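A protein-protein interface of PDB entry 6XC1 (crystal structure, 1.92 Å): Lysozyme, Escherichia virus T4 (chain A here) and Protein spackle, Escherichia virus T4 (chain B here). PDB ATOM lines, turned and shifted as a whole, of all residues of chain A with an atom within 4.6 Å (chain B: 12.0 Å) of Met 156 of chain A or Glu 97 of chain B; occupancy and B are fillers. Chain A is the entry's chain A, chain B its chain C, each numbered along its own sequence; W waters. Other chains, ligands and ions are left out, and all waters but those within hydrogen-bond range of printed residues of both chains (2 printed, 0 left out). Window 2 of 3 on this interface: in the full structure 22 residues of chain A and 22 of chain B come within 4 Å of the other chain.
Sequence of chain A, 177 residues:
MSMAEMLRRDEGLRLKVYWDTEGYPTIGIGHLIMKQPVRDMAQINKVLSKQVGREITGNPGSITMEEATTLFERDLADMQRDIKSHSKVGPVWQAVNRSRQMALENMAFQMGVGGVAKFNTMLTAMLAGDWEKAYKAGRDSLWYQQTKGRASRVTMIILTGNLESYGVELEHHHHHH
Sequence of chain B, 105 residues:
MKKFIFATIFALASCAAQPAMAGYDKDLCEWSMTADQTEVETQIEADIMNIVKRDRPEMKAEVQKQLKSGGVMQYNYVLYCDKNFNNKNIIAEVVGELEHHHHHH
NH2 of Arg 139 of chain A lies within salt-bridge range of OE2 of Glu 97 of chain B (3.0 Å).
The side-chain carboxylate of Glu 93 of chain B lies within salt-bridge range of the guanidinium group of Arg 153 of chain A (3.4 Å).
The side-chain hydroxyl of Tyr 135 of chain A sits at hydrogen-bond distance from the guanidinium group of Arg 139 of chain A.
NH2 of Arg 139 of chain A lies within hydrogen-bond range of O of Ser 152 of chain A (3.1 Å).
The side-chain hydroxyl (OG1) of Thr 155 of chain A is in hydrogen-bond range of the guanidinium group (NE) of Arg 139 of chain A (2.8 Å).
The backbone carbonyl oxygen (O) of Ser 152 of chain A is in hydrogen-bond range of the side-chain hydroxyl (OG1) of Thr 155 of chain A, at 3.3 Å.
OG of Ser 165 of chain A is in hydrogen-bond range of O of Arg 153 of chain A, at 2.8 Å.
O of Met 156 of chain A sits at hydrogen-bond distance from OG1 of Thr 160 of chain A (2.9 Å).
Ser 152 of chain A touches Gly 96 of chain B (OG to CA, 3.5 Å).
Glu 97 of chain B touches Ser 152 of chain A (OE1 to CB, 3.4 Å).
Met 156 of chain A touches Glu 97 of chain B (CE to OE2, 3.2 Å).
Of the printed residues of chain B, Arg 139 of chain A touches Glu 97.
Printed residues of chain B within 4 Å of Arg 153 of chain A: Glu 93.
Val 154 of chain A touches none of the printed residues of chain B.
No residue of chain B comes within 4 Å of Thr 155 of chain A.
Of chain B, only Glu 97 comes within 4 Å of Met 156 of chain A.
No residue of chain B comes within 4 Å of Ile 157 of chain A.
No residue of chain B comes within 4 Å of Ile 158 of chain A.
No residue of chain B comes within 4 Å of Leu 159 of chain A.
Glu 58 of chain B touches none of the printed residues of chain A.
Lys 88 of chain B touches none of the printed residues of chain A.
Printed residues of chain A within 4 Å of Glu 93 of chain B: Arg 153 (3.1 Å).
Of the printed residues of chain A, Glu 97 of chain B touches Arg 139, Ser 152 and Met 156.
The nearest residue of chain B that does not touch Met 156 of chain A is Gly 96 of chain B (8.3 Å).
The nearest printed residue of chain A that does not touch Gly 96 of chain B is Arg 153 of chain A (6.0 Å).
Printed residues of chain B that touch a printed residue of chain A: Glu 93, Gly 96 and Glu 97.
Of the 13 printed residues of chain A, 4 touch a printed residue of chain B.
Printed residues of chain A that touch a printed residue of chain B: Arg 139, Ser 152, Arg 153 and Met 156.
Along chain A the printed residues that touch a printed residue of chain B span positions 139 to 156.
Among the printed residues, Asp or Glu carboxylates within 4 Å of a Lys or Arg side-chain nitrogen of the other chain: Arg 139 of chain A with Glu 97 of chain B and Arg 153 of chain A with Glu 93 of chain B.
Water W2 bridges the backbone carbonyl oxygen of Ala 92 of chain B (2.5 Å) and the guanidinium group of Arg 153 of chain A (2.9 Å).
Water W1 lies within hydrogen-bond range of the side-chain hydroxyl of Ser 152 of chain A (2.6 Å), the side-chain carboxylate of Glu 97 of chain B (3.1 Å) and the guanidinium group of Arg 139 of chain A (3.5 Å).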
ATOM      1  N   TYR A 135      -2.594 -15.637 -25.123  1.00  0.00           N
ATOM      2  CA  TYR A 135      -2.206 -15.448 -23.729  1.00  0.00           C
ATOM      3  C   TYR A 135      -2.483 -16.698 -22.896  1.00  0.00           C
ATOM      4  O   TYR A 135      -1.623 -17.157 -22.135  1.00  0.00           O
ATOM      5  CB  TYR A 135      -2.958 -14.233 -23.179  1.00  0.00           C
ATOM      6  CG  TYR A 135      -2.808 -13.931 -21.704  1.00  0.00           C
ATOM      7  CD1 TYR A 135      -1.722 -13.204 -21.226  1.00  0.00           C
ATOM      8  CD2 TYR A 135      -3.788 -14.318 -20.795  1.00  0.00           C
ATOM      9  CE1 TYR A 135      -1.603 -12.902 -19.879  1.00  0.00           C
ATOM     10  CE2 TYR A 135      -3.679 -14.018 -19.451  1.00  0.00           C
ATOM     11  CZ  TYR A 135      -2.585 -13.311 -18.998  1.00  0.00           C
ATOM     12  OH  TYR A 135      -2.476 -13.013 -17.662  1.00  0.00           O
ATOM     13  N   ARG A 139       0.348 -19.229 -21.053  1.00  0.00           N
ATOM     14  CA  ARG A 139       0.373 -19.430 -19.609  1.00  0.00           C
ATOM     15  C   ARG A 139      -0.076 -20.826 -19.199  1.00  0.00           C
ATOM     16  O   ARG A 139       0.103 -21.200 -18.036  1.00  0.00           O
ATOM     17  CB  ARG A 139      -0.485 -18.371 -18.921  1.00  0.00           C
ATOM     18  CG  ARG A 139       0.057 -16.963 -19.123  1.00  0.00           C
ATOM     19  CD  ARG A 139      -0.340 -16.034 -18.002  1.00  0.00           C
ATOM     20  NE  ARG A 139       0.403 -14.778 -18.059  1.00  0.00           N
ATOM     21  CZ  ARG A 139       0.395 -13.863 -17.093  1.00  0.00           C
ATOM     22  NH1 ARG A 139      -0.326 -14.070 -15.996  1.00  0.00           N
ATOM     23  NH2 ARG A 139       1.097 -12.743 -17.227  1.00  0.00           N
ATOM     24  N   SER A 152       5.372 -14.492 -17.537  1.00  0.00           N
ATOM     25  CA  SER A 152       4.301 -13.536 -17.276  1.00  0.00           C
ATOM     26  C   SER A 152       4.532 -12.239 -18.040  1.00  0.00           C
ATOM     27  O   SER A 152       3.607 -11.691 -18.650  1.00  0.00           O
ATOM     28  CB  SER A 152       4.185 -13.255 -15.775  1.00  0.00           C
ATOM     29  OG  SER A 152       3.798 -14.424 -15.068  1.00  0.00           O
ATOM     30  N   ARG A 153       5.767 -11.729 -18.004  1.00  0.00           N
ATOM     31  CA  ARG A 153       6.094 -10.512 -18.743  1.00  0.00           C
ATOM     32  C   ARG A 153       5.887 -10.705 -20.236  1.00  0.00           C
ATOM     33  O   ARG A 153       5.327  -9.835 -20.913  1.00  0.00           O
ATOM     34  CB  ARG A 153       7.546 -10.101 -18.477  1.00  0.00           C
ATOM     35  CG  ARG A 153       7.844  -9.674 -17.064  1.00  0.00           C
ATOM     36  CD  ARG A 153       9.210  -8.996 -16.954  1.00  0.00           C
ATOM     37  NE  ARG A 153      10.333  -9.934 -16.996  1.00  0.00           N
ATOM     38  CZ  ARG A 153      10.671 -10.751 -16.001  1.00  0.00           C
ATOM     39  NH1 ARG A 153       9.961 -10.767 -14.880  1.00  0.00           N
ATOM     40  NH2 ARG A 153      11.722 -11.558 -16.127  1.00  0.00           N
ATOM     41  N   VAL A 154       6.332 -11.843 -20.769  1.00  0.00           N
ATOM     42  CA  VAL A 154       6.288 -12.055 -22.212  1.00  0.00           C
ATOM     43  C   VAL A 154       4.854 -12.271 -22.688  1.00  0.00           C
ATOM     44  O   VAL A 154       4.431 -11.689 -23.694  1.00  0.00           O
ATOM     45  CB  VAL A 154       7.208 -13.228 -22.597  1.00  0.00           C
ATOM     46  CG1 VAL A 154       7.040 -13.576 -24.066  1.00  0.00           C
ATOM     47  CG2 VAL A 154       8.670 -12.878 -22.278  1.00  0.00           C
ATOM     48  N   THR A 155       4.082 -13.099 -21.978  1.00  0.00           N
ATOM     49  CA  THR A 155       2.707 -13.347 -22.410  1.00  0.00           C
ATOM     50  C   THR A 155       1.849 -12.097 -22.274  1.00  0.00           C
ATOM     51  O   THR A 155       0.868 -11.940 -23.009  1.00  0.00           O
ATOM     52  CB  THR A 155       2.077 -14.510 -21.630  1.00  0.00           C
ATOM     53  OG1 THR A 155       2.188 -14.282 -20.218  1.00  0.00           O
ATOM     54  CG2 THR A 155       2.740 -15.839 -21.996  1.00  0.00           C
ATOM     55  N   MET A 156       2.207 -11.195 -21.356  1.00  0.00           N
ATOM     56  CA  MET A 156       1.465  -9.945 -21.232  1.00  0.00           C
ATOM     57  C   MET A 156       1.666  -9.060 -22.458  1.00  0.00           C
ATOM     58  O   MET A 156       0.742  -8.353 -22.877  1.00  0.00           O
ATOM     59  CB  MET A 156       1.880  -9.208 -19.959  1.00  0.00           C
ATOM     60  CG  MET A 156       0.957  -8.046 -19.596  1.00  0.00           C
ATOM     61  SD  MET A 156      -0.749  -8.559 -19.269  1.00  0.00           S
ATOM     62  CE  MET A 156      -0.500  -9.728 -17.942  1.00  0.00           C
ATOM     63  N   ILE A 157       2.867  -9.073 -23.043  1.00  0.00           N
ATOM     64  CA  ILE A 157       3.074  -8.387 -24.318  1.00  0.00           C
ATOM     65  C   ILE A 157       2.158  -8.975 -25.383  1.00  0.00           C
ATOM     66  O   ILE A 157       1.504  -8.250 -26.141  1.00  0.00           O
ATOM     67  CB  ILE A 157       4.549  -8.478 -24.748  1.00  0.00           C
ATOM     68  CG1 ILE A 157       5.466  -7.807 -23.724  1.00  0.00           C
ATOM     69  CG2 ILE A 157       4.740  -7.866 -26.142  1.00  0.00           C
ATOM     70  CD1 ILE A 157       6.926  -8.154 -23.938  1.00  0.00           C
ATOM     71  N   ILE A 158       2.106 -10.305 -25.452  1.00  0.00           N
ATOM     72  CA  ILE A 158       1.295 -10.980 -26.462  1.00  0.00           C
ATOM     73  C   ILE A 158      -0.173 -10.604 -26.304  1.00  0.00           C
ATOM     74  O   ILE A 158      -0.882 -10.366 -27.291  1.00  0.00           O
ATOM     75  CB  ILE A 158       1.514 -12.502 -26.373  1.00  0.00           C
ATOM     76  CG1 ILE A 158       2.932 -12.862 -26.833  1.00  0.00           C
ATOM     77  CG2 ILE A 158       0.461 -13.253 -27.178  1.00  0.00           C
ATOM     78  CD1 ILE A 158       3.266 -14.328 -26.686  1.00  0.00           C
ATOM     79  N   LEU A 159      -0.640 -10.510 -25.057  1.00  0.00           N
ATOM     80  CA  LEU A 159      -2.030 -10.149 -24.802  1.00  0.00           C
ATOM     81  C   LEU A 159      -2.311  -8.692 -25.157  1.00  0.00           C
ATOM     82  O   LEU A 159      -3.291  -8.390 -25.849  1.00  0.00           O
ATOM     83  CB  LEU A 159      -2.372 -10.420 -23.336  1.00  0.00           C
ATOM     84  CG  LEU A 159      -3.765  -9.976 -22.878  1.00  0.00           C
ATOM     85  CD1 LEU A 159      -4.848 -10.654 -23.702  1.00  0.00           C
ATOM     86  CD2 LEU A 159      -3.952 -10.268 -21.400  1.00  0.00           C
ATOM     87  N   THR A 160      -1.470  -7.769 -24.681  1.00  0.00           N
ATOM     88  CA  THR A 160      -1.785  -6.346 -24.749  1.00  0.00           C
ATOM     89  C   THR A 160      -1.241  -5.653 -25.989  1.00  0.00           C
ATOM     90  O   THR A 160      -1.787  -4.619 -26.387  1.00  0.00           O
ATOM     91  CB  THR A 160      -1.242  -5.615 -23.518  1.00  0.00           C
ATOM     92  OG1 THR A 160       0.191  -5.626 -23.556  1.00  0.00           O
ATOM     93  CG2 THR A 160      -1.729  -6.281 -22.228  1.00  0.00           C
ATOM     94  N   GLY A 161      -0.174  -6.166 -26.591  1.00  0.00           N
ATOM     95  CA  GLY A 161       0.406  -5.520 -27.747  1.00  0.00           C
ATOM     96  C   GLY A 161       1.386  -4.405 -27.447  1.00  0.00           C
ATOM     97  O   GLY A 161       1.885  -3.774 -28.390  1.00  0.00           O
ATOM     98  N   SER A 165       4.619  -4.281 -19.611  1.00  0.00           N
ATOM     99  CA  SER A 165       5.049  -5.292 -18.648  1.00  0.00           C
ATOM    100  C   SER A 165       6.552  -5.257 -18.413  1.00  0.00           C
ATOM    101  O   SER A 165       7.033  -5.864 -17.449  1.00  0.00           O
ATOM    102  CB  SER A 165       4.619  -6.692 -19.101  1.00  0.00           C
ATOM    103  OG  SER A 165       5.335  -7.130 -20.244  1.00  0.00           O
ATOM    104  N   ARG B  56       6.025  -9.991   1.370  1.00  0.00           N
ATOM    105  CA  ARG B  56       5.020 -10.966   0.935  1.00  0.00           C
ATOM    106  C   ARG B  56       5.409 -12.352   1.424  1.00  0.00           C
ATOM    107  O   ARG B  56       5.730 -13.242   0.625  1.00  0.00           O
ATOM    108  CB  ARG B  56       4.881 -10.954  -0.590  1.00  0.00           C
ATOM    109  CG  ARG B  56       4.232  -9.716  -1.179  1.00  0.00           C
ATOM    110  CD  ARG B  56       2.772  -9.617  -0.775  1.00  0.00           C
ATOM    111  NE  ARG B  56       1.993  -8.845  -1.736  1.00  0.00           N
ATOM    112  CZ  ARG B  56       1.311  -9.379  -2.743  1.00  0.00           C
ATOM    113  NH1 ARG B  56       0.631  -8.599  -3.571  1.00  0.00           N
ATOM    114  NH2 ARG B  56       1.307 -10.693  -2.921  1.00  0.00           N
ATOM    115  N   GLU B  58       3.914 -14.955   2.275  1.00  0.00           N
ATOM    116  CA  GLU B  58       3.201 -16.104   1.725  1.00  0.00           C
ATOM    117  C   GLU B  58       3.750 -16.548   0.372  1.00  0.00           C
ATOM    118  O   GLU B  58       3.440 -17.659  -0.071  1.00  0.00           O
ATOM    119  CB  GLU B  58       1.707 -15.789   1.596  1.00  0.00           C
ATOM    120  CG  GLU B  58       1.338 -14.905   0.407  1.00  0.00           C
ATOM    121  CD  GLU B  58       1.592 -13.424   0.649  1.00  0.00           C
ATOM    122  OE1 GLU B  58       1.318 -12.622  -0.268  1.00  0.00           O
ATOM    123  OE2 GLU B  58       2.058 -13.056   1.750  1.00  0.00           O
ATOM    124  N   MET B  59       4.546 -15.711  -0.298  1.00  0.00           N
ATOM    125  CA  MET B  59       5.122 -16.068  -1.590  1.00  0.00           C
ATOM    126  C   MET B  59       6.411 -16.872  -1.466  1.00  0.00           C
ATOM    127  O   MET B  59       7.033 -17.177  -2.492  1.00  0.00           O
ATOM    128  CB  MET B  59       5.392 -14.808  -2.417  1.00  0.00           C
ATOM    129  CG  MET B  59       4.158 -13.967  -2.716  1.00  0.00           C
ATOM    130  SD  MET B  59       2.857 -14.862  -3.591  1.00  0.00           S
ATOM    131  CE  MET B  59       3.773 -15.644  -4.920  1.00  0.00           C
ATOM    132  N   GLU B  62       6.499 -20.270  -3.429  1.00  0.00           N
ATOM    133  CA  GLU B  62       6.489 -20.056  -4.874  1.00  0.00           C
ATOM    134  C   GLU B  62       7.826 -19.501  -5.359  1.00  0.00           C
ATOM    135  O   GLU B  62       8.335 -19.915  -6.408  1.00  0.00           O
ATOM    136  CB  GLU B  62       5.346 -19.114  -5.251  1.00  0.00           C
ATOM    137  CG  GLU B  62       5.175 -18.896  -6.755  1.00  0.00           C
ATOM    138  CD  GLU B  62       4.796 -20.157  -7.494  1.00  0.00           C
ATOM    139  OE1 GLU B  62       4.233 -21.070  -6.864  1.00  0.00           O
ATOM    140  OE2 GLU B  62       5.062 -20.236  -8.705  1.00  0.00           O
ATOM    141  N   VAL B  63       8.403 -18.561  -4.610  1.00  0.00           N
ATOM    142  CA  VAL B  63       9.700 -17.997  -4.980  1.00  0.00           C
ATOM    143  C   VAL B  63      10.766 -19.085  -4.991  1.00  0.00           C
ATOM    144  O   VAL B  63      11.561 -19.191  -5.933  1.00  0.00           O
ATOM    145  CB  VAL B  63      10.078 -16.850  -4.026  1.00  0.00           C
ATOM    146  CG1 VAL B  63      11.542 -16.448  -4.226  1.00  0.00           C
ATOM    147  CG2 VAL B  63       9.159 -15.662  -4.241  1.00  0.00           C
ATOM    148  N   GLN B  66      10.366 -21.250  -7.999  1.00  0.00           N
ATOM    149  CA  GLN B  66      10.780 -20.576  -9.226  1.00  0.00           C
ATOM    150  C   GLN B  66      12.299 -20.455  -9.318  1.00  0.00           C
ATOM    151  O   GLN B  66      12.867 -20.573 -10.410  1.00  0.00           O
ATOM    152  CB  GLN B  66      10.126 -19.200  -9.315  1.00  0.00           C
ATOM    153  CG  GLN B  66       8.647 -19.250  -9.647  1.00  0.00           C
ATOM    154  CD  GLN B  66       8.378 -19.994 -10.933  1.00  0.00           C
ATOM    155  OE1 GLN B  66       9.083 -19.810 -11.934  1.00  0.00           O
ATOM    156  NE2 GLN B  66       7.358 -20.848 -10.918  1.00  0.00           N
ATOM    157  N   TYR B  75      19.034 -12.592 -12.114  1.00  0.00           N
ATOM    158  CA  TYR B  75      18.522 -11.406 -11.441  1.00  0.00           C
ATOM    159  C   TYR B  75      19.623 -10.463 -10.981  1.00  0.00           C
ATOM    160  O   TYR B  75      19.317  -9.440 -10.357  1.00  0.00           O
ATOM    161  CB  TYR B  75      17.647 -11.826 -10.251  1.00  0.00           C
ATOM    162  CG  TYR B  75      16.536 -12.764 -10.673  1.00  0.00           C
ATOM    163  CD1 TYR B  75      15.456 -12.300 -11.418  1.00  0.00           C
ATOM    164  CD2 TYR B  75      16.576 -14.116 -10.349  1.00  0.00           C
ATOM    165  CE1 TYR B  75      14.438 -13.156 -11.823  1.00  0.00           C
ATOM    166  CE2 TYR B  75      15.559 -14.982 -10.744  1.00  0.00           C
ATOM    167  CZ  TYR B  75      14.497 -14.498 -11.484  1.00  0.00           C
ATOM    168  OH  TYR B  75      13.482 -15.354 -11.881  1.00  0.00           O
ATOM    169  N   PHE B  85      15.486   0.038 -11.434  1.00  0.00           N
ATOM    170  CA  PHE B  85      14.690  -1.074 -10.935  1.00  0.00           C
ATOM    171  C   PHE B  85      14.577  -0.960  -9.421  1.00  0.00           C
ATOM    172  O   PHE B  85      15.591  -0.852  -8.724  1.00  0.00           O
ATOM    173  CB  PHE B  85      15.309  -2.419 -11.329  1.00  0.00           C
ATOM    174  CG  PHE B  85      14.444  -3.612 -10.994  1.00  0.00           C
ATOM    175  CD1 PHE B  85      13.476  -4.060 -11.883  1.00  0.00           C
ATOM    176  CD2 PHE B  85      14.606  -4.291  -9.793  1.00  0.00           C
ATOM    177  CE1 PHE B  85      12.680  -5.166 -11.578  1.00  0.00           C
ATOM    178  CE2 PHE B  85      13.817  -5.393  -9.483  1.00  0.00           C
ATOM    179  CZ  PHE B  85      12.851  -5.831 -10.377  1.00  0.00           C
ATOM    180  N   LYS B  88      12.009  -3.839  -4.457  1.00  0.00           N
ATOM    181  CA  LYS B  88      10.751  -4.347  -3.912  1.00  0.00           C
ATOM    182  C   LYS B  88       9.981  -5.149  -4.955  1.00  0.00           C
ATOM    183  O   LYS B  88       9.219  -6.057  -4.602  1.00  0.00           O
ATOM    184  CB  LYS B  88       9.884  -3.197  -3.393  1.00  0.00           C
ATOM    185  CG  LYS B  88       9.243  -2.364  -4.498  1.00  0.00           C
ATOM    186  CD  LYS B  88       8.218  -1.371  -3.968  1.00  0.00           C
ATOM    187  CE  LYS B  88       7.588  -0.585  -5.114  1.00  0.00           C
ATOM    188  NZ  LYS B  88       6.542   0.369  -4.654  1.00  0.00           N
ATOM    189  N   ASN B  89      10.175  -4.836  -6.237  1.00  0.00           N
ATOM    190  CA  ASN B  89       9.511  -5.506  -7.345  1.00  0.00           C
ATOM    191  C   ASN B  89      10.192  -6.811  -7.745  1.00  0.00           C
ATOM    192  O   ASN B  89       9.809  -7.402  -8.764  1.00  0.00           O
ATOM    193  CB  ASN B  89       9.437  -4.565  -8.555  1.00  0.00           C
ATOM    194  CG  ASN B  89       8.664  -3.293  -8.257  1.00  0.00           C
ATOM    195  OD1 ASN B  89       7.666  -3.316  -7.535  1.00  0.00           O
ATOM    196  ND2 ASN B  89       9.120  -2.171  -8.813  1.00  0.00           N
ATOM    197  N   ILE B  90      11.185  -7.276  -6.977  1.00  0.00           N
ATOM    198  CA  ILE B  90      11.874  -8.509  -7.344  1.00  0.00           C
ATOM    199  C   ILE B  90      10.955  -9.714  -7.181  1.00  0.00           C
ATOM    200  O   ILE B  90      11.117 -10.723  -7.880  1.00  0.00           O
ATOM    201  CB  ILE B  90      13.172  -8.683  -6.533  1.00  0.00           C
ATOM    202  CG1 ILE B  90      14.081  -9.705  -7.220  1.00  0.00           C
ATOM    203  CG2 ILE B  90      12.879  -9.106  -5.099  1.00  0.00           C
ATOM    204  CD1 ILE B  90      14.556  -9.266  -8.592  1.00  0.00           C
ATOM    205  N   ILE B  91       9.980  -9.639  -6.272  1.00  0.00           N
ATOM    206  CA  ILE B  91       9.058 -10.759  -6.095  1.00  0.00           C
ATOM    207  C   ILE B  91       8.275 -11.000  -7.377  1.00  0.00           C
ATOM    208  O   ILE B  91       8.233 -12.123  -7.898  1.00  0.00           O
ATOM    209  CB  ILE B  91       8.125 -10.513  -4.896  1.00  0.00           C
ATOM    210  CG1 ILE B  91       8.939 -10.189  -3.638  1.00  0.00           C
ATOM    211  CG2 ILE B  91       7.247 -11.729  -4.661  1.00  0.00           C
ATOM    212  CD1 ILE B  91       8.089 -10.044  -2.391  1.00  0.00           C
ATOM    213  N   ALA B  92       7.669  -9.940  -7.926  1.00  0.00           N
ATOM    214  CA  ALA B  92       6.957 -10.063  -9.194  1.00  0.00           C
ATOM    215  C   ALA B  92       7.901 -10.390 -10.350  1.00  0.00           C
ATOM    216  O   ALA B  92       7.476 -10.979 -11.348  1.00  0.00           O
ATOM    217  CB  ALA B  92       6.178  -8.781  -9.489  1.00  0.00           C
ATOM    218  N   GLU B  93       9.178 -10.020 -10.240  1.00  0.00           N
ATOM    219  CA  GLU B  93      10.129 -10.392 -11.286  1.00  0.00           C
ATOM    220  C   GLU B  93      10.344 -11.901 -11.326  1.00  0.00           C
ATOM    221  O   GLU B  93      10.555 -12.469 -12.403  1.00  0.00           O
ATOM    222  CB  GLU B  93      11.463  -9.673 -11.073  1.00  0.00           C
ATOM    223  CG  GLU B  93      12.414  -9.741 -12.270  1.00  0.00           C
ATOM    224  CD  GLU B  93      12.063  -8.756 -13.368  1.00  0.00           C
ATOM    225  OE1 GLU B  93      11.116  -7.958 -13.193  1.00  0.00           O
ATOM    226  OE2 GLU B  93      12.742  -8.773 -14.421  1.00  0.00           O
ATOM    227  N   VAL B  94      10.268 -12.561 -10.169  1.00  0.00           N
ATOM    228  CA  VAL B  94      10.505 -13.998 -10.090  1.00  0.00           C
ATOM    229  C   VAL B  94       9.236 -14.791 -10.402  1.00  0.00           C
ATOM    230  O   VAL B  94       9.283 -15.783 -11.138  1.00  0.00           O
ATOM    231  CB  VAL B  94      11.074 -14.358  -8.703  1.00  0.00           C
ATOM    232  CG1 VAL B  94      11.072 -15.864  -8.493  1.00  0.00           C
ATOM    233  CG2 VAL B  94      12.496 -13.795  -8.530  1.00  0.00           C
ATOM    234  N   VAL B  95       8.087 -14.387  -9.854  1.00  0.00           N
ATOM    235  CA  VAL B  95       6.879 -15.210  -9.911  1.00  0.00           C
ATOM    236  C   VAL B  95       5.789 -14.616 -10.789  1.00  0.00           C
ATOM    237  O   VAL B  95       4.749 -15.269 -10.984  1.00  0.00           O
ATOM    238  CB  VAL B  95       6.320 -15.496  -8.501  1.00  0.00           C
ATOM    239  CG1 VAL B  95       7.394 -16.070  -7.610  1.00  0.00           C
ATOM    240  CG2 VAL B  95       5.722 -14.234  -7.893  1.00  0.00           C
ATOM    241  N   GLY B  96       5.977 -13.414 -11.322  1.00  0.00           N
ATOM    242  CA  GLY B  96       4.974 -12.784 -12.155  1.00  0.00           C
ATOM    243  C   GLY B  96       4.109 -11.812 -11.368  1.00  0.00           C
ATOM    244  O   GLY B  96       4.166 -11.723 -10.138  1.00  0.00           O
ATOM    245  N   GLU B  97       3.285 -11.073 -12.110  1.00  0.00           N
ATOM    246  CA  GLU B  97       2.551  -9.957 -11.526  1.00  0.00           C
ATOM    247  C   GLU B  97       1.688 -10.424 -10.359  1.00  0.00           C
ATOM    248  O   GLU B  97       1.098 -11.507 -10.391  1.00  0.00           O
ATOM    249  CB  GLU B  97       1.692  -9.266 -12.587  1.00  0.00           C
ATOM    250  CG  GLU B  97       0.437 -10.019 -13.015  1.00  0.00           C
ATOM    251  CD  GLU B  97       0.696 -11.056 -14.092  1.00  0.00           C
ATOM    252  OE1 GLU B  97       1.674 -11.821 -13.973  1.00  0.00           O
ATOM    253  OE2 GLU B  97      -0.087 -11.106 -15.065  1.00  0.00           O
ATOM    254  N   LEU B  98       1.648  -9.607  -9.309  1.00  0.00           N
ATOM    255  CA  LEU B  98       0.937  -9.952  -8.083  1.00  0.00           C
ATOM    256  C   LEU B  98      -0.429  -9.268  -8.034  1.00  0.00           C
ATOM    257  O   LEU B  98      -1.125  -9.316  -7.019  1.00  0.00           O
ATOM    258  CB  LEU B  98       1.767  -9.563  -6.856  1.00  0.00           C
ATOM    259  CG  LEU B  98       3.217 -10.062  -6.783  1.00  0.00           C
ATOM    260  CD1 LEU B  98       3.915  -9.483  -5.567  1.00  0.00           C
ATOM    261  CD2 LEU B  98       3.287 -11.579  -6.754  1.00  0.00           C
HETATM  262  O   HOH W   1       1.878 -14.862 -13.421  1.00  0.00           O
HETATM  263  O   HOH W   2       7.454 -10.045 -13.717  1.00  0.00           O
